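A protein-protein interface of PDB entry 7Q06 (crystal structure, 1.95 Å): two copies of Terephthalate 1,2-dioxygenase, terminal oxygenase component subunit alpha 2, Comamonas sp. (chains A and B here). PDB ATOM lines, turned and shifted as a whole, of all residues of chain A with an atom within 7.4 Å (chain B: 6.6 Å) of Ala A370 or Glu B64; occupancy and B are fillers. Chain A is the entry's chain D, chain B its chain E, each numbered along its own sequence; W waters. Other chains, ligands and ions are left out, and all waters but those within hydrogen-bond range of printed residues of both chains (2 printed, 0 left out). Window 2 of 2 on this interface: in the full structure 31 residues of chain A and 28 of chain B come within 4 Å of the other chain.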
ATOM      1  N   THR A  24     -23.559   7.555 -15.904  1.00  0.00           N
ATOM      2  CA  THR A  24     -24.110   8.832 -16.437  1.00  0.00           C
ATOM      3  C   THR A  24     -24.330   8.797 -17.954  1.00  0.00           C
ATOM      4  O   THR A  24     -25.008   9.689 -18.473  1.00  0.00           O
ATOM      5  CB  THR A  24     -23.249  10.038 -16.082  1.00  0.00           C
ATOM      6  OG1 THR A  24     -21.889   9.831 -16.490  1.00  0.00           O
ATOM      7  CG2 THR A  24     -23.288  10.337 -14.605  1.00  0.00           C
ATOM      8  N   PHE A 364     -24.779   9.706  -2.713  1.00  0.00           N
ATOM      9  CA  PHE A 364     -23.473  10.274  -2.303  1.00  0.00           C
ATOM     10  C   PHE A 364     -22.460   9.921  -3.389  1.00  0.00           C
ATOM     11  O   PHE A 364     -21.622  10.782  -3.669  1.00  0.00           O
ATOM     12  CB  PHE A 364     -23.053   9.792  -0.922  1.00  0.00           C
ATOM     13  CG  PHE A 364     -23.996  10.190   0.192  1.00  0.00           C
ATOM     14  CD1 PHE A 364     -24.874  11.246   0.058  1.00  0.00           C
ATOM     15  CD2 PHE A 364     -23.953   9.516   1.392  1.00  0.00           C
ATOM     16  CE1 PHE A 364     -25.683  11.637   1.111  1.00  0.00           C
ATOM     17  CE2 PHE A 364     -24.769   9.898   2.451  1.00  0.00           C
ATOM     18  CZ  PHE A 364     -25.649  10.941   2.295  1.00  0.00           C
ATOM     19  N   VAL A 365     -22.550   8.732  -3.988  1.00  0.00           N
ATOM     20  CA  VAL A 365     -21.630   8.338  -5.089  1.00  0.00           C
ATOM     21  C   VAL A 365     -21.982   9.180  -6.332  1.00  0.00           C
ATOM     22  O   VAL A 365     -21.071   9.820  -6.972  1.00  0.00           O
ATOM     23  CB  VAL A 365     -21.667   6.816  -5.360  1.00  0.00           C
ATOM     24  CG1 VAL A 365     -20.761   6.452  -6.543  1.00  0.00           C
ATOM     25  CG2 VAL A 365     -21.227   6.037  -4.120  1.00  0.00           C
ATOM     26  N   GLN A 366     -23.257   9.186  -6.703  1.00  0.00           N
ATOM     27  CA  GLN A 366     -23.716   9.912  -7.925  1.00  0.00           C
ATOM     28  C   GLN A 366     -23.173  11.344  -7.869  1.00  0.00           C
ATOM     29  O   GLN A 366     -22.672  11.835  -8.868  1.00  0.00           O
ATOM     30  CB  GLN A 366     -25.250   9.829  -8.024  1.00  0.00           C
ATOM     31  CG  GLN A 366     -25.807  10.219  -9.391  1.00  0.00           C
ATOM     32  CD  GLN A 366     -25.830   9.062 -10.374  1.00  0.00           C
ATOM     33  OE1 GLN A 366     -26.145   7.913 -10.032  1.00  0.00           O
ATOM     34  NE2 GLN A 366     -25.473   9.351 -11.623  1.00  0.00           N
ATOM     35  N   ARG A 367     -23.215  11.988  -6.705  1.00  0.00           N
ATOM     36  CA  ARG A 367     -22.781  13.379  -6.537  1.00  0.00           C
ATOM     37  C   ARG A 367     -21.270  13.467  -6.391  1.00  0.00           C
ATOM     38  O   ARG A 367     -20.652  14.471  -6.910  1.00  0.00           O
ATOM     39  CB  ARG A 367     -23.495  14.006  -5.354  1.00  0.00           C
ATOM     40  CG  ARG A 367     -24.929  14.403  -5.687  1.00  0.00           C
ATOM     41  CD  ARG A 367     -25.885  14.455  -4.504  1.00  0.00           C
ATOM     42  NE  ARG A 367     -25.408  15.427  -3.534  1.00  0.00           N
ATOM     43  CZ  ARG A 367     -25.880  15.538  -2.310  1.00  0.00           C
ATOM     44  NH1 ARG A 367     -25.408  16.454  -1.469  1.00  0.00           N
ATOM     45  NH2 ARG A 367     -26.746  14.639  -1.893  1.00  0.00           N
ATOM     46  N   GLY A 368     -20.663  12.541  -5.665  1.00  0.00           N
ATOM     47  CA  GLY A 368     -19.221  12.546  -5.457  1.00  0.00           C
ATOM     48  C   GLY A 368     -18.422  12.459  -6.764  1.00  0.00           C
ATOM     49  O   GLY A 368     -17.273  12.979  -6.818  1.00  0.00           O
ATOM     50  N   ILE A 369     -18.975  11.834  -7.795  1.00  0.00           N
ATOM     51  CA  ILE A 369     -18.268  11.605  -9.080  1.00  0.00           C
ATOM     52  C   ILE A 369     -18.616  12.711 -10.082  1.00  0.00           C
ATOM     53  O   ILE A 369     -18.256  12.551 -11.259  1.00  0.00           O
ATOM     54  CB  ILE A 369     -18.568  10.203  -9.648  1.00  0.00           C
ATOM     55  CG1 ILE A 369     -20.041  10.020 -10.036  1.00  0.00           C
ATOM     56  CG2 ILE A 369     -18.075   9.142  -8.671  1.00  0.00           C
ATOM     57  CD1 ILE A 369     -20.375   8.666 -10.603  1.00  0.00           C
ATOM     58  N   ALA A 370     -19.318  13.766  -9.686  1.00  0.00           N
ATOM     59  CA  ALA A 370     -19.884  14.745 -10.663  1.00  0.00           C
ATOM     60  C   ALA A 370     -18.752  15.348 -11.516  1.00  0.00           C
ATOM     61  O   ALA A 370     -19.016  15.641 -12.673  1.00  0.00           O
ATOM     62  CB  ALA A 370     -20.687  15.816  -9.934  1.00  0.00           C
ATOM     63  N   GLY A 371     -17.540  15.562 -10.976  1.00  0.00           N
ATOM     64  CA  GLY A 371     -16.386  16.044 -11.774  1.00  0.00           C
ATOM     65  C   GLY A 371     -15.440  14.970 -12.296  1.00  0.00           C
ATOM     66  O   GLY A 371     -14.285  15.309 -12.643  1.00  0.00           O
ATOM     67  N   ALA A 372     -15.838  13.700 -12.290  1.00  0.00           N
ATOM     68  CA  ALA A 372     -14.900  12.559 -12.401  1.00  0.00           C
ATOM     69  C   ALA A 372     -15.429  11.524 -13.413  1.00  0.00           C
ATOM     70  O   ALA A 372     -15.076  10.347 -13.259  1.00  0.00           O
ATOM     71  CB  ALA A 372     -14.700  11.931 -11.034  1.00  0.00           C
ATOM     72  N   ALA A 373     -16.254  11.915 -14.391  1.00  0.00           N
ATOM     73  CA  ALA A 373     -16.844  10.980 -15.385  1.00  0.00           C
ATOM     74  C   ALA A 373     -15.717  10.185 -16.081  1.00  0.00           C
ATOM     75  O   ALA A 373     -16.022   9.032 -16.486  1.00  0.00           O
ATOM     76  CB  ALA A 373     -17.720  11.720 -16.382  1.00  0.00           C
ATOM     77  N   ALA B  29     -20.493  22.799 -22.375  1.00  0.00           N
ATOM     78  CA  ALA B  29     -20.578  22.949 -20.896  1.00  0.00           C
ATOM     79  C   ALA B  29     -19.580  21.970 -20.262  1.00  0.00           C
ATOM     80  O   ALA B  29     -18.870  22.369 -19.317  1.00  0.00           O
ATOM     81  CB  ALA B  29     -21.990  22.707 -20.403  1.00  0.00           C
ATOM     82  N   ASP B  30     -19.500  20.742 -20.776  1.00  0.00           N
ATOM     83  CA  ASP B  30     -18.555  19.731 -20.233  1.00  0.00           C
ATOM     84  C   ASP B  30     -17.109  20.194 -20.494  1.00  0.00           C
ATOM     85  O   ASP B  30     -16.253  20.042 -19.582  1.00  0.00           O
ATOM     86  CB  ASP B  30     -18.823  18.320 -20.754  1.00  0.00           C
ATOM     87  CG  ASP B  30     -17.905  17.311 -20.068  1.00  0.00           C
ATOM     88  OD1 ASP B  30     -17.923  17.243 -18.830  1.00  0.00           O
ATOM     89  OD2 ASP B  30     -17.111  16.689 -20.763  1.00  0.00           O
ATOM     90  N   GLN B  33     -16.024  22.622 -17.846  1.00  0.00           N
ATOM     91  CA  GLN B  33     -15.616  21.956 -16.585  1.00  0.00           C
ATOM     92  C   GLN B  33     -14.150  21.515 -16.683  1.00  0.00           C
ATOM     93  O   GLN B  33     -13.400  21.787 -15.728  1.00  0.00           O
ATOM     94  CB  GLN B  33     -16.562  20.804 -16.298  1.00  0.00           C
ATOM     95  CG  GLN B  33     -17.998  21.272 -16.085  1.00  0.00           C
ATOM     96  CD  GLN B  33     -18.227  22.132 -14.859  1.00  0.00           C
ATOM     97  OE1 GLN B  33     -17.442  22.182 -13.910  1.00  0.00           O
ATOM     98  NE2 GLN B  33     -19.377  22.784 -14.857  1.00  0.00           N
ATOM     99  N   GLN B  34     -13.767  20.915 -17.808  1.00  0.00           N
ATOM    100  CA  GLN B  34     -12.381  20.443 -18.028  1.00  0.00           C
ATOM    101  C   GLN B  34     -11.427  21.621 -18.224  1.00  0.00           C
ATOM    102  O   GLN B  34     -10.388  21.615 -17.603  1.00  0.00           O
ATOM    103  CB  GLN B  34     -12.326  19.526 -19.241  1.00  0.00           C
ATOM    104  CG  GLN B  34     -13.165  18.255 -19.056  1.00  0.00           C
ATOM    105  CD  GLN B  34     -13.086  17.396 -20.296  1.00  0.00           C
ATOM    106  OE1 GLN B  34     -11.993  17.175 -20.791  1.00  0.00           O
ATOM    107  NE2 GLN B  34     -14.225  16.913 -20.777  1.00  0.00           N
ATOM    108  N   TYR B  37     -13.000  25.305 -15.149  1.00  0.00           N
ATOM    109  CA  TYR B  37     -13.096  25.124 -13.689  1.00  0.00           C
ATOM    110  C   TYR B  37     -11.939  24.244 -13.176  1.00  0.00           C
ATOM    111  O   TYR B  37     -11.355  24.596 -12.093  1.00  0.00           O
ATOM    112  CB  TYR B  37     -14.503  24.656 -13.334  1.00  0.00           C
ATOM    113  CG  TYR B  37     -15.577  25.702 -13.577  1.00  0.00           C
ATOM    114  CD1 TYR B  37     -15.675  26.841 -12.809  1.00  0.00           C
ATOM    115  CD2 TYR B  37     -16.516  25.533 -14.580  1.00  0.00           C
ATOM    116  CE1 TYR B  37     -16.701  27.762 -12.958  1.00  0.00           C
ATOM    117  CE2 TYR B  37     -17.514  26.480 -14.805  1.00  0.00           C
ATOM    118  CZ  TYR B  37     -17.615  27.592 -13.984  1.00  0.00           C
ATOM    119  OH  TYR B  37     -18.627  28.470 -14.186  1.00  0.00           O
ATOM    120  N   ARG B  38     -11.577  23.191 -13.920  1.00  0.00           N
ATOM    121  CA  ARG B  38     -10.441  22.285 -13.567  1.00  0.00           C
ATOM    122  C   ARG B  38      -9.186  22.665 -14.379  1.00  0.00           C
ATOM    123  O   ARG B  38      -8.223  21.933 -14.302  1.00  0.00           O
ATOM    124  CB  ARG B  38     -10.840  20.805 -13.691  1.00  0.00           C
ATOM    125  CG  ARG B  38     -11.974  20.415 -12.738  1.00  0.00           C
ATOM    126  CD  ARG B  38     -12.116  18.897 -12.646  1.00  0.00           C
ATOM    127  NE  ARG B  38     -12.542  18.231 -13.899  1.00  0.00           N
ATOM    128  CZ  ARG B  38     -13.761  18.121 -14.354  1.00  0.00           C
ATOM    129  NH1 ARG B  38     -13.953  17.511 -15.510  1.00  0.00           N
ATOM    130  NH2 ARG B  38     -14.798  18.639 -13.706  1.00  0.00           N
ATOM    131  N   PHE B  61     -17.996  24.119  -4.088  1.00  0.00           N
ATOM    132  CA  PHE B  61     -17.821  23.548  -5.433  1.00  0.00           C
ATOM    133  C   PHE B  61     -16.787  24.414  -6.150  1.00  0.00           C
ATOM    134  O   PHE B  61     -16.623  25.593  -5.810  1.00  0.00           O
ATOM    135  CB  PHE B  61     -19.107  23.554  -6.233  1.00  0.00           C
ATOM    136  CG  PHE B  61     -20.132  22.519  -5.846  1.00  0.00           C
ATOM    137  CD1 PHE B  61     -21.059  22.791  -4.879  1.00  0.00           C
ATOM    138  CD2 PHE B  61     -20.202  21.292  -6.513  1.00  0.00           C
ATOM    139  CE1 PHE B  61     -22.036  21.846  -4.531  1.00  0.00           C
ATOM    140  CE2 PHE B  61     -21.175  20.346  -6.189  1.00  0.00           C
ATOM    141  CZ  PHE B  61     -22.123  20.643  -5.225  1.00  0.00           C
ATOM    142  N   ALA B  62     -16.038  23.769  -7.030  1.00  0.00           N
ATOM    143  CA  ALA B  62     -15.270  24.420  -8.089  1.00  0.00           C
ATOM    144  C   ALA B  62     -15.922  23.961  -9.400  1.00  0.00           C
ATOM    145  O   ALA B  62     -15.779  22.806  -9.796  1.00  0.00           O
ATOM    146  CB  ALA B  62     -13.807  24.078  -7.938  1.00  0.00           C
ATOM    147  N   GLY B  63     -16.660  24.836 -10.043  1.00  0.00           N
ATOM    148  CA  GLY B  63     -17.556  24.406 -11.148  1.00  0.00           C
ATOM    149  C   GLY B  63     -18.525  23.355 -10.603  1.00  0.00           C
ATOM    150  O   GLY B  63     -19.114  23.592  -9.523  1.00  0.00           O
ATOM    151  N   GLU B  64     -18.631  22.221 -11.293  1.00  0.00           N
ATOM    152  CA  GLU B  64     -19.511  21.082 -10.913  1.00  0.00           C
ATOM    153  C   GLU B  64     -18.834  20.246  -9.795  1.00  0.00           C
ATOM    154  O   GLU B  64     -19.470  19.299  -9.312  1.00  0.00           O
ATOM    155  CB  GLU B  64     -19.767  20.179 -12.125  1.00  0.00           C
ATOM    156  CG  GLU B  64     -18.535  19.312 -12.533  1.00  0.00           C
ATOM    157  CD  GLU B  64     -18.560  18.625 -13.915  1.00  0.00           C
ATOM    158  OE1 GLU B  64     -19.660  18.541 -14.469  1.00  0.00           O
ATOM    159  OE2 GLU B  64     -17.455  18.162 -14.464  1.00  0.00           O
ATOM    160  N   THR B  65     -17.554  20.469  -9.491  1.00  0.00           N
ATOM    161  CA  THR B  65     -16.743  19.518  -8.670  1.00  0.00           C
ATOM    162  C   THR B  65     -16.837  19.889  -7.204  1.00  0.00           C
ATOM    163  O   THR B  65     -16.498  21.005  -6.813  1.00  0.00           O
ATOM    164  CB  THR B  65     -15.292  19.421  -9.131  1.00  0.00           C
ATOM    165  OG1 THR B  65     -15.257  19.120 -10.537  1.00  0.00           O
ATOM    166  CG2 THR B  65     -14.586  18.326  -8.353  1.00  0.00           C
ATOM    167  N   PRO B  66     -17.378  19.022  -6.327  1.00  0.00           N
ATOM    168  CA  PRO B  66     -17.489  19.365  -4.899  1.00  0.00           C
ATOM    169  C   PRO B  66     -16.082  19.408  -4.275  1.00  0.00           C
ATOM    170  O   PRO B  66     -15.246  18.601  -4.631  1.00  0.00           O
ATOM    171  CB  PRO B  66     -18.353  18.237  -4.330  1.00  0.00           C
ATOM    172  CG  PRO B  66     -18.006  17.066  -5.249  1.00  0.00           C
ATOM    173  CD  PRO B  66     -17.883  17.671  -6.631  1.00  0.00           C
ATOM    174  N   GLU B  81     -10.788  17.742  -3.574  1.00  0.00           N
ATOM    175  CA  GLU B  81     -12.029  17.249  -4.176  1.00  0.00           C
ATOM    176  C   GLU B  81     -12.754  16.368  -3.147  1.00  0.00           C
ATOM    177  O   GLU B  81     -12.131  15.443  -2.573  1.00  0.00           O
ATOM    178  CB  GLU B  81     -11.690  16.493  -5.450  1.00  0.00           C
ATOM    179  CG  GLU B  81     -12.909  15.958  -6.197  1.00  0.00           C
ATOM    180  CD  GLU B  81     -12.479  15.190  -7.436  1.00  0.00           C
ATOM    181  OE1 GLU B  81     -11.221  14.976  -7.561  1.00  0.00           O
ATOM    182  OE2 GLU B  81     -13.382  14.772  -8.252  1.00  0.00           O
ATOM    183  N   ARG B  83     -14.410  13.653  -2.958  1.00  0.00           N
ATOM    184  CA  ARG B  83     -14.665  12.395  -3.715  1.00  0.00           C
ATOM    185  C   ARG B  83     -13.761  11.318  -3.107  1.00  0.00           C
ATOM    186  O   ARG B  83     -12.542  11.428  -3.189  1.00  0.00           O
ATOM    187  CB  ARG B  83     -14.408  12.532  -5.224  1.00  0.00           C
ATOM    188  CG  ARG B  83     -14.569  11.235  -5.991  1.00  0.00           C
ATOM    189  CD  ARG B  83     -14.319  11.289  -7.505  1.00  0.00           C
ATOM    190  NE  ARG B  83     -13.081  11.993  -7.810  1.00  0.00           N
ATOM    191  CZ  ARG B  83     -11.872  11.428  -7.851  1.00  0.00           C
ATOM    192  NH1 ARG B  83     -10.800  12.154  -8.020  1.00  0.00           N
ATOM    193  NH2 ARG B  83     -11.704  10.149  -7.663  1.00  0.00           N
ATOM    194  N   GLY B  88     -16.177   6.542  -4.900  1.00  0.00           N
ATOM    195  CA  GLY B  88     -16.477   7.913  -5.383  1.00  0.00           C
ATOM    196  C   GLY B  88     -17.500   8.675  -4.527  1.00  0.00           C
ATOM    197  O   GLY B  88     -17.885   9.788  -4.924  1.00  0.00           O
ATOM    198  N   LEU B 314     -21.722  29.743  -9.292  1.00  0.00           N
ATOM    199  CA  LEU B 314     -21.458  28.325  -9.638  1.00  0.00           C
ATOM    200  C   LEU B 314     -22.382  27.909 -10.754  1.00  0.00           C
ATOM    201  O   LEU B 314     -23.566  28.211 -10.735  1.00  0.00           O
ATOM    202  CB  LEU B 314     -21.660  27.411  -8.430  1.00  0.00           C
ATOM    203  CG  LEU B 314     -20.805  27.705  -7.200  1.00  0.00           C
ATOM    204  CD1 LEU B 314     -21.285  26.836  -6.027  1.00  0.00           C
ATOM    205  CD2 LEU B 314     -19.343  27.411  -7.514  1.00  0.00           C
ATOM    206  N   PRO B 315     -21.884  27.108 -11.715  1.00  0.00           N
ATOM    207  CA  PRO B 315     -22.745  26.534 -12.748  1.00  0.00           C
ATOM    208  C   PRO B 315     -23.539  25.412 -12.065  1.00  0.00           C
ATOM    209  O   PRO B 315     -22.971  24.783 -11.175  1.00  0.00           O
ATOM    210  CB  PRO B 315     -21.743  26.040 -13.786  1.00  0.00           C
ATOM    211  CG  PRO B 315     -20.554  25.683 -12.997  1.00  0.00           C
ATOM    212  CD  PRO B 315     -20.491  26.678 -11.859  1.00  0.00           C
ATOM    213  N   LYS B 316     -24.794  25.191 -12.448  1.00  0.00           N
ATOM    214  CA  LYS B 316     -25.547  24.035 -11.942  1.00  0.00           C
ATOM    215  C   LYS B 316     -26.009  23.109 -13.074  1.00  0.00           C
ATOM    216  O   LYS B 316     -25.975  21.904 -12.864  1.00  0.00           O
ATOM    217  CB  LYS B 316     -26.680  24.481 -11.002  1.00  0.00           C
ATOM    218  CG  LYS B 316     -26.108  24.973  -9.658  1.00  0.00           C
ATOM    219  CD  LYS B 316     -25.344  23.895  -8.845  1.00  0.00           C
ATOM    220  CE  LYS B 316     -24.867  24.496  -7.539  1.00  0.00           C
ATOM    221  NZ  LYS B 316     -23.873  23.651  -6.845  1.00  0.00           N
HETATM  222  O   HOH W   1     -16.170  14.865  -8.582  1.00  0.00           O
HETATM  223  O   HOH W   2     -12.176  14.861 -14.319  1.00  0.00           O
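The backbone carbonyl oxygen (O) of Ala A370 lies close to the side-chain carboxylate (OE2) of Glu B64.
Water W2 lies within hydrogen-bond range of O of Gly A371 (2.7 Å) and NH1 of Arg B38 (3.4 Å). Water W1 lies within hydrogen-bond range of the backbone carbonyl oxygen (O) of Gly A368 (2.8 Å), the side-chain carboxylate (OE2) of Glu B81 (2.8 Å) and the backbone NH (N) of Gly A371 (2.8 Å).
Among the printed residues, pairs that only touch across the chains: Gly A368 with Gly B88, Gly A368 with Arg B83, Gly A371 with Arg B38, Gly A371 with Thr B65, Gly A371 with Glu B64, Ala A372 with Arg B83, Ile A369 with Gly B88 and Val A365 with Gly B88.
Printed residues of chain B within 4 Å of Val A365: Gly B88. Of the printed residues of chain B, Gly A368 touches Arg B83 (3.3 Å) and Gly B88 (3.1 Å). Ala A370 touches just one residue of chain B: Glu B64 (3.3 Å). Printed residues of chain B within 4 Å of Ala A372: Arg B83. Phe B61 touches none of the printed residues of chain A. The nearest residue of chain B that does not touch Ala A370 is Pro B66 (4.7 Å). The nearest residue of chain A that does not touch Glu B64 is Ala A372 (5.2 Å). The nearest printed residue of chain B that does not touch Val A365 is Arg B83 (6.7 Å).
The backbone carbonyl oxygen (O) of Gln B33 lies within hydrogen-bond range of the backbone NH (N) of Arg B38, at 2.9 Å. The guanidinium group of Arg B38 is in hydrogen-bond range of the side-chain hydroxyl of Thr B65, at 3.2 Å. The side-chain amide oxygen (OE1) of Gln B33 lies within hydrogen-bond range of the backbone NH (N) of Glu B64 (2.9 Å). The side-chain carboxylate of Glu B81 is in salt-bridge range of the guanidinium group of Arg B83, 2.8 Å away. NH2 of Arg B38 is in salt-bridge range of OE2 of Glu B64, at 2.8 Å.
No position is printed for both chains.
Of the 18 printed residues of chain B, 5 touch a printed residue of chain A. Printed residues of chain B that touch a printed residue of chain A: Arg B38, Glu B64, Thr B65, Arg B83 and Gly B88. Printed residues of chain A that touch a printed residue of chain B: Val A365, Gly A368, Ile A369, Ala A370, Gly A371 and Ala A372. Hydrophobic or aromatic side chains of chain A within 4 Å of the printed part of chain B: Ile A369, Ala A370 and Ala A372. Among the printed residues, 9 pairs touch across the chains.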
